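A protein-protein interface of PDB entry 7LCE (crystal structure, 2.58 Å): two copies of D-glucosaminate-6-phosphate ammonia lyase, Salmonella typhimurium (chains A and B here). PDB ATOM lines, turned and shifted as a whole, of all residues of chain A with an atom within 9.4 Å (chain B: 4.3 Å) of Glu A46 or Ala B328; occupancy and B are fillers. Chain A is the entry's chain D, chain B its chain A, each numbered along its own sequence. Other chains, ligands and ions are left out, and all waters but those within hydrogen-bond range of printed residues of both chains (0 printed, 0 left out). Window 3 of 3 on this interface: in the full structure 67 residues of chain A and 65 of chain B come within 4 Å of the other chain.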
ATOM      1  N   ALA A  43      23.583   4.461 -11.345  1.00  0.00           N
ATOM      2  CA  ALA A  43      22.147   4.298 -11.516  1.00  0.00           C
ATOM      3  C   ALA A  43      21.494   4.133 -10.154  1.00  0.00           C
ATOM      4  O   ALA A  43      22.122   3.688  -9.191  1.00  0.00           O
ATOM      5  CB  ALA A  43      21.812   3.104 -12.417  1.00  0.00           C
ATOM      6  N   PHE A  44      20.218   4.490 -10.090  1.00  0.00           N
ATOM      7  CA  PHE A  44      19.440   4.349  -8.872  1.00  0.00           C
ATOM      8  C   PHE A  44      18.756   2.987  -8.836  1.00  0.00           C
ATOM      9  O   PHE A  44      18.560   2.332  -9.863  1.00  0.00           O
ATOM     10  CB  PHE A  44      18.400   5.465  -8.767  1.00  0.00           C
ATOM     11  CG  PHE A  44      18.994   6.824  -8.554  1.00  0.00           C
ATOM     12  CD1 PHE A  44      19.343   7.251  -7.287  1.00  0.00           C
ATOM     13  CD2 PHE A  44      19.209   7.674  -9.625  1.00  0.00           C
ATOM     14  CE1 PHE A  44      19.896   8.503  -7.089  1.00  0.00           C
ATOM     15  CE2 PHE A  44      19.759   8.928  -9.433  1.00  0.00           C
ATOM     16  CZ  PHE A  44      20.103   9.342  -8.163  1.00  0.00           C
ATOM     17  N   VAL A  45      18.395   2.563  -7.626  1.00  0.00           N
ATOM     18  CA  VAL A  45      17.736   1.277  -7.433  1.00  0.00           C
ATOM     19  C   VAL A  45      16.950   1.348  -6.136  1.00  0.00           C
ATOM     20  O   VAL A  45      17.331   2.052  -5.198  1.00  0.00           O
ATOM     21  CB  VAL A  45      18.761   0.113  -7.422  1.00  0.00           C
ATOM     22  CG1 VAL A  45      19.704   0.234  -6.237  1.00  0.00           C
ATOM     23  CG2 VAL A  45      18.048  -1.231  -7.414  1.00  0.00           C
ATOM     24  N   GLU A  46      15.839   0.621  -6.091  1.00  0.00           N
ATOM     25  CA  GLU A  46      15.079   0.466  -4.858  1.00  0.00           C
ATOM     26  C   GLU A  46      15.871  -0.443  -3.924  1.00  0.00           C
ATOM     27  O   GLU A  46      15.959  -1.652  -4.156  1.00  0.00           O
ATOM     28  CB  GLU A  46      13.704  -0.112  -5.175  1.00  0.00           C
ATOM     29  CG  GLU A  46      12.930   0.699  -6.209  1.00  0.00           C
ATOM     30  CD  GLU A  46      11.594   0.080  -6.575  1.00  0.00           C
ATOM     31  OE1 GLU A  46      11.520  -1.166  -6.673  1.00  0.00           O
ATOM     32  OE2 GLU A  46      10.620   0.837  -6.773  1.00  0.00           O
ATOM     33  N   ILE A  47      16.457   0.139  -2.872  1.00  0.00           N
ATOM     34  CA  ILE A  47      17.426  -0.597  -2.059  1.00  0.00           C
ATOM     35  C   ILE A  47      16.777  -1.812  -1.406  1.00  0.00           C
ATOM     36  O   ILE A  47      17.395  -2.879  -1.306  1.00  0.00           O
ATOM     37  CB  ILE A  47      18.077   0.334  -1.019  1.00  0.00           C
ATOM     38  CG1 ILE A  47      18.975   1.357  -1.713  1.00  0.00           C
ATOM     39  CG2 ILE A  47      18.907  -0.462  -0.027  1.00  0.00           C
ATOM     40  CD1 ILE A  47      20.305   0.777  -2.170  1.00  0.00           C
ATOM     41  N   ASP A  48      15.521  -1.680  -0.968  1.00  0.00           N
ATOM     42  CA  ASP A  48      14.842  -2.808  -0.335  1.00  0.00           C
ATOM     43  C   ASP A  48      14.785  -4.010  -1.272  1.00  0.00           C
ATOM     44  O   ASP A  48      14.937  -5.157  -0.834  1.00  0.00           O
ATOM     45  CB  ASP A  48      13.435  -2.402   0.105  1.00  0.00           C
ATOM     46  CG  ASP A  48      12.566  -1.949  -1.053  1.00  0.00           C
ATOM     47  OD1 ASP A  48      13.117  -1.430  -2.048  1.00  0.00           O
ATOM     48  OD2 ASP A  48      11.331  -2.119  -0.973  1.00  0.00           O
ATOM     49  N   ALA A  49      14.573  -3.765  -2.566  1.00  0.00           N
ATOM     50  CA  ALA A  49      14.571  -4.856  -3.534  1.00  0.00           C
ATOM     51  C   ALA A  49      15.982  -5.358  -3.817  1.00  0.00           C
ATOM     52  O   ALA A  49      16.175  -6.556  -4.054  1.00  0.00           O
ATOM     53  CB  ALA A  49      13.895  -4.407  -4.828  1.00  0.00           C
ATOM     54  N   LEU A  50      16.975  -4.462  -3.801  1.00  0.00           N
ATOM     55  CA  LEU A  50      18.358  -4.879  -4.015  1.00  0.00           C
ATOM     56  C   LEU A  50      18.862  -5.728  -2.854  1.00  0.00           C
ATOM     57  O   LEU A  50      19.611  -6.689  -3.060  1.00  0.00           O
ATOM     58  CB  LEU A  50      19.251  -3.655  -4.219  1.00  0.00           C
ATOM     59  CG  LEU A  50      20.721  -3.918  -4.556  1.00  0.00           C
ATOM     60  CD1 LEU A  50      20.860  -4.663  -5.877  1.00  0.00           C
ATOM     61  CD2 LEU A  50      21.504  -2.616  -4.591  1.00  0.00           C
ATOM     62  N   VAL A  51      18.470  -5.381  -1.624  1.00  0.00           N
ATOM     63  CA  VAL A  51      18.865  -6.171  -0.460  1.00  0.00           C
ATOM     64  C   VAL A  51      18.308  -7.584  -0.569  1.00  0.00           C
ATOM     65  O   VAL A  51      19.000  -8.567  -0.272  1.00  0.00           O
ATOM     66  CB  VAL A  51      18.408  -5.480   0.840  1.00  0.00           C
ATOM     67  CG1 VAL A  51      18.542  -6.422   2.023  1.00  0.00           C
ATOM     68  CG2 VAL A  51      19.209  -4.207   1.084  1.00  0.00           C
ATOM     69  N   GLU A  52      17.048  -7.711  -0.994  1.00  0.00           N
ATOM     70  CA  GLU A  52      16.431  -9.028  -1.114  1.00  0.00           C
ATOM     71  C   GLU A  52      17.059  -9.840  -2.241  1.00  0.00           C
ATOM     72  O   GLU A  52      17.393 -11.016  -2.057  1.00  0.00           O
ATOM     73  CB  GLU A  52      14.925  -8.883  -1.326  1.00  0.00           C
ATOM     74  CG  GLU A  52      14.192  -8.322  -0.122  1.00  0.00           C
ATOM     75  CD  GLU A  52      14.106  -9.321   1.017  1.00  0.00           C
ATOM     76  OE1 GLU A  52      13.439 -10.366   0.845  1.00  0.00           O
ATOM     77  OE2 GLU A  52      14.711  -9.063   2.078  1.00  0.00           O
ATOM     78  N   LYS A  53      17.224  -9.233  -3.419  1.00  0.00           N
ATOM     79  CA  LYS A  53      17.747  -9.983  -4.559  1.00  0.00           C
ATOM     80  C   LYS A  53      19.190 -10.413  -4.330  1.00  0.00           C
ATOM     81  O   LYS A  53      19.554 -11.561  -4.616  1.00  0.00           O
ATOM     82  CB  LYS A  53      17.631  -9.159  -5.840  1.00  0.00           C
ATOM     83  CG  LYS A  53      17.910  -9.951  -7.115  1.00  0.00           C
ATOM     84  CD  LYS A  53      16.923 -11.088  -7.324  1.00  0.00           C
ATOM     85  CE  LYS A  53      15.596 -10.583  -7.870  1.00  0.00           C
ATOM     86  NZ  LYS A  53      14.640 -11.694  -8.144  1.00  0.00           N
ATOM     87  N   THR A  54      20.027  -9.514  -3.804  1.00  0.00           N
ATOM     88  CA  THR A  54      21.417  -9.880  -3.547  1.00  0.00           C
ATOM     89  C   THR A  54      21.509 -10.994  -2.512  1.00  0.00           C
ATOM     90  O   THR A  54      22.366 -11.879  -2.613  1.00  0.00           O
ATOM     91  CB  THR A  54      22.216  -8.659  -3.096  1.00  0.00           C
ATOM     92  OG1 THR A  54      21.513  -7.988  -2.044  1.00  0.00           O
ATOM     93  CG2 THR A  54      22.417  -7.702  -4.257  1.00  0.00           C
ATOM     94  N   LYS A 248      25.066   0.510  -2.813  1.00  0.00           N
ATOM     95  CA  LYS A 248      24.525  -0.318  -3.883  1.00  0.00           C
ATOM     96  C   LYS A 248      25.616  -0.769  -4.845  1.00  0.00           C
ATOM     97  O   LYS A 248      25.505  -1.843  -5.449  1.00  0.00           O
ATOM     98  CB  LYS A 248      23.432   0.444  -4.630  1.00  0.00           C
ATOM     99  CG  LYS A 248      23.830   1.856  -5.028  1.00  0.00           C
ATOM    100  CD  LYS A 248      22.733   2.542  -5.824  1.00  0.00           C
ATOM    101  CE  LYS A 248      23.113   3.975  -6.172  1.00  0.00           C
ATOM    102  NZ  LYS A 248      24.473   4.077  -6.770  1.00  0.00           N
ATOM    103  N   MET A 251      27.487  -3.784  -3.269  1.00  0.00           N
ATOM    104  CA  MET A 251      26.552  -4.901  -3.199  1.00  0.00           C
ATOM    105  C   MET A 251      26.508  -5.649  -4.524  1.00  0.00           C
ATOM    106  O   MET A 251      26.604  -6.882  -4.562  1.00  0.00           O
ATOM    107  CB  MET A 251      25.162  -4.397  -2.815  1.00  0.00           C
ATOM    108  CG  MET A 251      25.025  -4.024  -1.351  1.00  0.00           C
ATOM    109  SD  MET A 251      23.415  -3.306  -0.982  1.00  0.00           S
ATOM    110  CE  MET A 251      22.343  -4.716  -1.247  1.00  0.00           C
ATOM    111  N   LYS B  12      13.549  -2.995 -10.882  1.00  0.00           N
ATOM    112  CA  LYS B  12      12.965  -1.936 -11.691  1.00  0.00           C
ATOM    113  C   LYS B  12      13.994  -0.867 -12.033  1.00  0.00           C
ATOM    114  O   LYS B  12      14.887  -0.553 -11.241  1.00  0.00           O
ATOM    115  CB  LYS B  12      11.796  -1.280 -10.959  1.00  0.00           C
ATOM    116  CG  LYS B  12      10.717  -2.232 -10.506  1.00  0.00           C
ATOM    117  CD  LYS B  12       9.700  -1.504  -9.650  1.00  0.00           C
ATOM    118  CE  LYS B  12       8.355  -1.449 -10.339  1.00  0.00           C
ATOM    119  NZ  LYS B  12       7.326  -0.802  -9.483  1.00  0.00           N
ATOM    120  N   LYS B  13      13.858  -0.304 -13.230  1.00  0.00           N
ATOM    121  CA  LYS B  13      14.595   0.907 -13.560  1.00  0.00           C
ATOM    122  C   LYS B  13      13.999   2.075 -12.785  1.00  0.00           C
ATOM    123  O   LYS B  13      12.787   2.305 -12.830  1.00  0.00           O
ATOM    124  CB  LYS B  13      14.541   1.174 -15.062  1.00  0.00           C
ATOM    125  CG  LYS B  13      15.150   2.498 -15.479  1.00  0.00           C
ATOM    126  CD  LYS B  13      15.121   2.677 -16.988  1.00  0.00           C
ATOM    127  CE  LYS B  13      15.662   4.042 -17.375  1.00  0.00           C
ATOM    128  NZ  LYS B  13      17.063   4.222 -16.900  1.00  0.00           N
ATOM    129  N   VAL B  14      14.845   2.812 -12.074  1.00  0.00           N
ATOM    130  CA  VAL B  14      14.404   3.882 -11.186  1.00  0.00           C
ATOM    131  C   VAL B  14      14.785   5.222 -11.796  1.00  0.00           C
ATOM    132  O   VAL B  14      15.920   5.405 -12.256  1.00  0.00           O
ATOM    133  CB  VAL B  14      15.009   3.729  -9.780  1.00  0.00           C
ATOM    134  CG1 VAL B  14      14.553   4.867  -8.884  1.00  0.00           C
ATOM    135  CG2 VAL B  14      14.627   2.384  -9.182  1.00  0.00           C
ATOM    136  N   ILE B  15      13.840   6.158 -11.793  1.00  0.00           N
ATOM    137  CA  ILE B  15      14.082   7.538 -12.194  1.00  0.00           C
ATOM    138  C   ILE B  15      13.872   8.411 -10.966  1.00  0.00           C
ATOM    139  O   ILE B  15      12.758   8.479 -10.431  1.00  0.00           O
ATOM    140  CB  ILE B  15      13.159   7.979 -13.339  1.00  0.00           C
ATOM    141  CG1 ILE B  15      13.326   7.062 -14.548  1.00  0.00           C
ATOM    142  CG2 ILE B  15      13.444   9.424 -13.725  1.00  0.00           C
ATOM    143  CD1 ILE B  15      12.508   7.493 -15.745  1.00  0.00           C
ATOM    144  N   ILE B  23      16.684   5.685   0.334  1.00  0.00           N
ATOM    145  CA  ILE B  23      15.951   4.502  -0.118  1.00  0.00           C
ATOM    146  C   ILE B  23      16.184   4.192  -1.588  1.00  0.00           C
ATOM    147  O   ILE B  23      15.742   3.139  -2.067  1.00  0.00           O
ATOM    148  CB  ILE B  23      14.434   4.633   0.121  1.00  0.00           C
ATOM    149  CG1 ILE B  23      13.803   5.552  -0.919  1.00  0.00           C
ATOM    150  CG2 ILE B  23      14.158   5.158   1.517  1.00  0.00           C
ATOM    151  CD1 ILE B  23      12.299   5.639  -0.815  1.00  0.00           C
ATOM    152  N   LEU B 322       3.240   6.821 -10.470  1.00  0.00           N
ATOM    153  CA  LEU B 322       4.595   7.066 -10.952  1.00  0.00           C
ATOM    154  C   LEU B 322       5.589   6.095 -10.324  1.00  0.00           C
ATOM    155  O   LEU B 322       6.454   5.551 -11.019  1.00  0.00           O
ATOM    156  CB  LEU B 322       5.000   8.508 -10.663  1.00  0.00           C
ATOM    157  CG  LEU B 322       4.341   9.557 -11.555  1.00  0.00           C
ATOM    158  CD1 LEU B 322       4.627  10.951 -11.029  1.00  0.00           C
ATOM    159  CD2 LEU B 322       4.839   9.408 -12.982  1.00  0.00           C
ATOM    160  N   ARG B 323       5.479   5.862  -9.012  1.00  0.00           N
ATOM    161  CA  ARG B 323       6.386   4.929  -8.350  1.00  0.00           C
ATOM    162  C   ARG B 323       6.051   3.483  -8.691  1.00  0.00           C
ATOM    163  O   ARG B 323       6.951   2.677  -8.953  1.00  0.00           O
ATOM    164  CB  ARG B 323       6.338   5.128  -6.837  1.00  0.00           C
ATOM    165  CG  ARG B 323       6.838   6.471  -6.354  1.00  0.00           C
ATOM    166  CD  ARG B 323       6.705   6.566  -4.848  1.00  0.00           C
ATOM    167  NE  ARG B 323       5.324   6.365  -4.429  1.00  0.00           N
ATOM    168  CZ  ARG B 323       4.920   6.315  -3.166  1.00  0.00           C
ATOM    169  NH1 ARG B 323       5.772   6.452  -2.164  1.00  0.00           N
ATOM    170  NH2 ARG B 323       3.632   6.122  -2.904  1.00  0.00           N
ATOM    171  N   GLY B 325       4.661   2.083 -11.253  1.00  0.00           N
ATOM    172  CA  GLY B 325       4.767   1.642 -12.632  1.00  0.00           C
ATOM    173  C   GLY B 325       5.990   0.775 -12.870  1.00  0.00           C
ATOM    174  O   GLY B 325       6.871   0.623 -12.026  1.00  0.00           O
ATOM    175  N   GLU B 326       6.032   0.188 -14.071  1.00  0.00           N
ATOM    176  CA  GLU B 326       7.157  -0.666 -14.445  1.00  0.00           C
ATOM    177  C   GLU B 326       8.472   0.104 -14.402  1.00  0.00           C
ATOM    178  O   GLU B 326       9.520  -0.473 -14.085  1.00  0.00           O
ATOM    179  CB  GLU B 326       6.909  -1.274 -15.827  1.00  0.00           C
ATOM    180  CG  GLU B 326       7.914  -2.333 -16.245  1.00  0.00           C
ATOM    181  CD  GLU B 326       7.809  -2.689 -17.716  1.00  0.00           C
ATOM    182  OE1 GLU B 326       6.971  -2.083 -18.418  1.00  0.00           O
ATOM    183  OE2 GLU B 326       8.553  -3.586 -18.164  1.00  0.00           O
ATOM    184  N   ILE B 327       8.438   1.394 -14.721  1.00  0.00           N
ATOM    185  CA  ILE B 327       9.555   2.299 -14.482  1.00  0.00           C
ATOM    186  C   ILE B 327       9.210   3.088 -13.225  1.00  0.00           C
ATOM    187  O   ILE B 327       8.268   3.889 -13.225  1.00  0.00           O
ATOM    188  CB  ILE B 327       9.806   3.231 -15.675  1.00  0.00           C
ATOM    189  CG1 ILE B 327      10.140   2.429 -16.933  1.00  0.00           C
ATOM    190  CG2 ILE B 327      10.932   4.202 -15.356  1.00  0.00           C
ATOM    191  CD1 ILE B 327      11.371   1.565 -16.800  1.00  0.00           C
ATOM    192  N   ALA B 328       9.956   2.855 -12.147  1.00  0.00           N
ATOM    193  CA  ALA B 328       9.693   3.503 -10.865  1.00  0.00           C
ATOM    194  C   ALA B 328      10.155   4.955 -10.920  1.00  0.00           C
ATOM    195  O   ALA B 328      11.358   5.228 -10.973  1.00  0.00           O
ATOM    196  CB  ALA B 328      10.395   2.751  -9.740  1.00  0.00           C
ATOM    197  N   ILE B 329       9.205   5.888 -10.903  1.00  0.00           N
ATOM    198  CA  ILE B 329       9.491   7.318 -10.965  1.00  0.00           C
ATOM    199  C   ILE B 329       9.169   7.936  -9.611  1.00  0.00           C
ATOM    200  O   ILE B 329       8.009   7.936  -9.178  1.00  0.00           O
ATOM    201  CB  ILE B 329       8.703   8.009 -12.088  1.00  0.00           C
ATOM    202  CG1 ILE B 329       9.110   7.449 -13.452  1.00  0.00           C
ATOM    203  CG2 ILE B 329       8.911   9.512 -12.036  1.00  0.00           C
ATOM    204  CD1 ILE B 329       8.109   7.728 -14.545  1.00  0.00           C
ATOM    205  N   TYR B 330      10.196   8.461  -8.943  1.00  0.00           N
ATOM    206  CA  TYR B 330      10.066   9.046  -7.612  1.00  0.00           C
ATOM    207  C   TYR B 330      10.116  10.565  -7.733  1.00  0.00           C
ATOM    208  O   TYR B 330      11.167  11.136  -8.046  1.00  0.00           O
ATOM    209  CB  TYR B 330      11.166   8.529  -6.687  1.00  0.00           C
ATOM    210  CG  TYR B 330      10.991   7.084  -6.272  1.00  0.00           C
ATOM    211  CD1 TYR B 330      11.423   6.048  -7.089  1.00  0.00           C
ATOM    212  CD2 TYR B 330      10.396   6.757  -5.060  1.00  0.00           C
ATOM    213  CE1 TYR B 330      11.264   4.727  -6.713  1.00  0.00           C
ATOM    214  CE2 TYR B 330      10.234   5.438  -4.676  1.00  0.00           C
ATOM    215  CZ  TYR B 330      10.669   4.427  -5.505  1.00  0.00           C
ATOM    216  OH  TYR B 330      10.509   3.110  -5.125  1.00  0.00           O
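CB of Val B14 touches O of Phe A44, 3.8 Å away.
Val A45 touches Val B14.
Val A45 touches Ile B23 (O to O, 3.7 Å).
OE1 of Glu A46 touches CD of Lys B12, 3.5 Å away.
Val B14 touches Glu A46.
Ile B23 touches Glu A46 (O to CA, 3.9 Å).
Ala B328 touches Glu A46 (CB to OE2, 3.5 Å).
Of the 13 printed residues of chain B, 5 touch a printed residue of chain A.
Printed residues of chain B that touch a printed residue of chain A: Lys B12, Val B14, Ile B23, Ala B328 and Tyr B330.
Printed residues of chain A that touch a printed residue of chain B: Phe A44, Val A45, Glu A46 and Ile A47.
Among the printed residues, 9 pairs touch across the chains.
Among the printed residues, no Asp or Glu carboxylate lies within 4 Å of a Lys or Arg side-chain nitrogen of the other chain.
No position is printed for both chains.
Of the printed residues of chain B, Val A45 touches Val B14 (3.7 Å) and Ile B23 (3.7 Å).
Of the printed residues of chain B, Glu A46 touches Lys B12 (3.5 Å), Val B14 (3.8 Å), Ile B23 (3.9 Å), Ala B328 (3.5 Å) and Tyr B330 (2.8 Å).
Printed residues of chain B within 4 Å of Ile A47: Ile B23 (3.2 Å).
Of the printed residues of chain A, Lys B12 touches Glu A46 (3.5 Å).
Val B14 touches three residues of chain A.
Of the printed residues of chain A, Ile B23 touches Val A45, Glu A46 and Ile A47.
Gly B325 touches none of the printed residues of chain A.
Ile B327 touches none of the printed residues of chain A.
Of chain A, only Glu A46 comes within 4 Å of Ala B328.
No residue of chain A comes within 4 Å of Ile B329.
The nearest printed residue of chain B that does not touch Glu A46 is Arg B323 (4.6 Å).
The nearest residue of chain A that does not touch Ala B328 is Phe A44 (7.4 Å).
The nearest printed residue of chain A that does not touch Ile B23 is Asp A48 (4.9 Å).
N of Ile A47 lies within hydrogen-bond range of O of Ile B23 (3.2 Å).
The side-chain hydroxyl of Tyr B330 lies within hydrogen-bond range of the side-chain carboxylate of Glu A46 (2.8 Å).
The side-chain amino group (NZ) of Lys B12 is in hydrogen-bond range of the backbone carbonyl oxygen (O) of Gly B325, at 3.0 Å.
N of Ala B328 sits at hydrogen-bond distance from O of Lys B13 (3.0 Å).
N of Ile B15 is in hydrogen-bond range of O of Ala B328, at 2.8 Å.
The backbone NH (N) of Tyr B330 is in hydrogen-bond range of the backbone carbonyl oxygen (O) of Ile B15 (3.0 Å).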
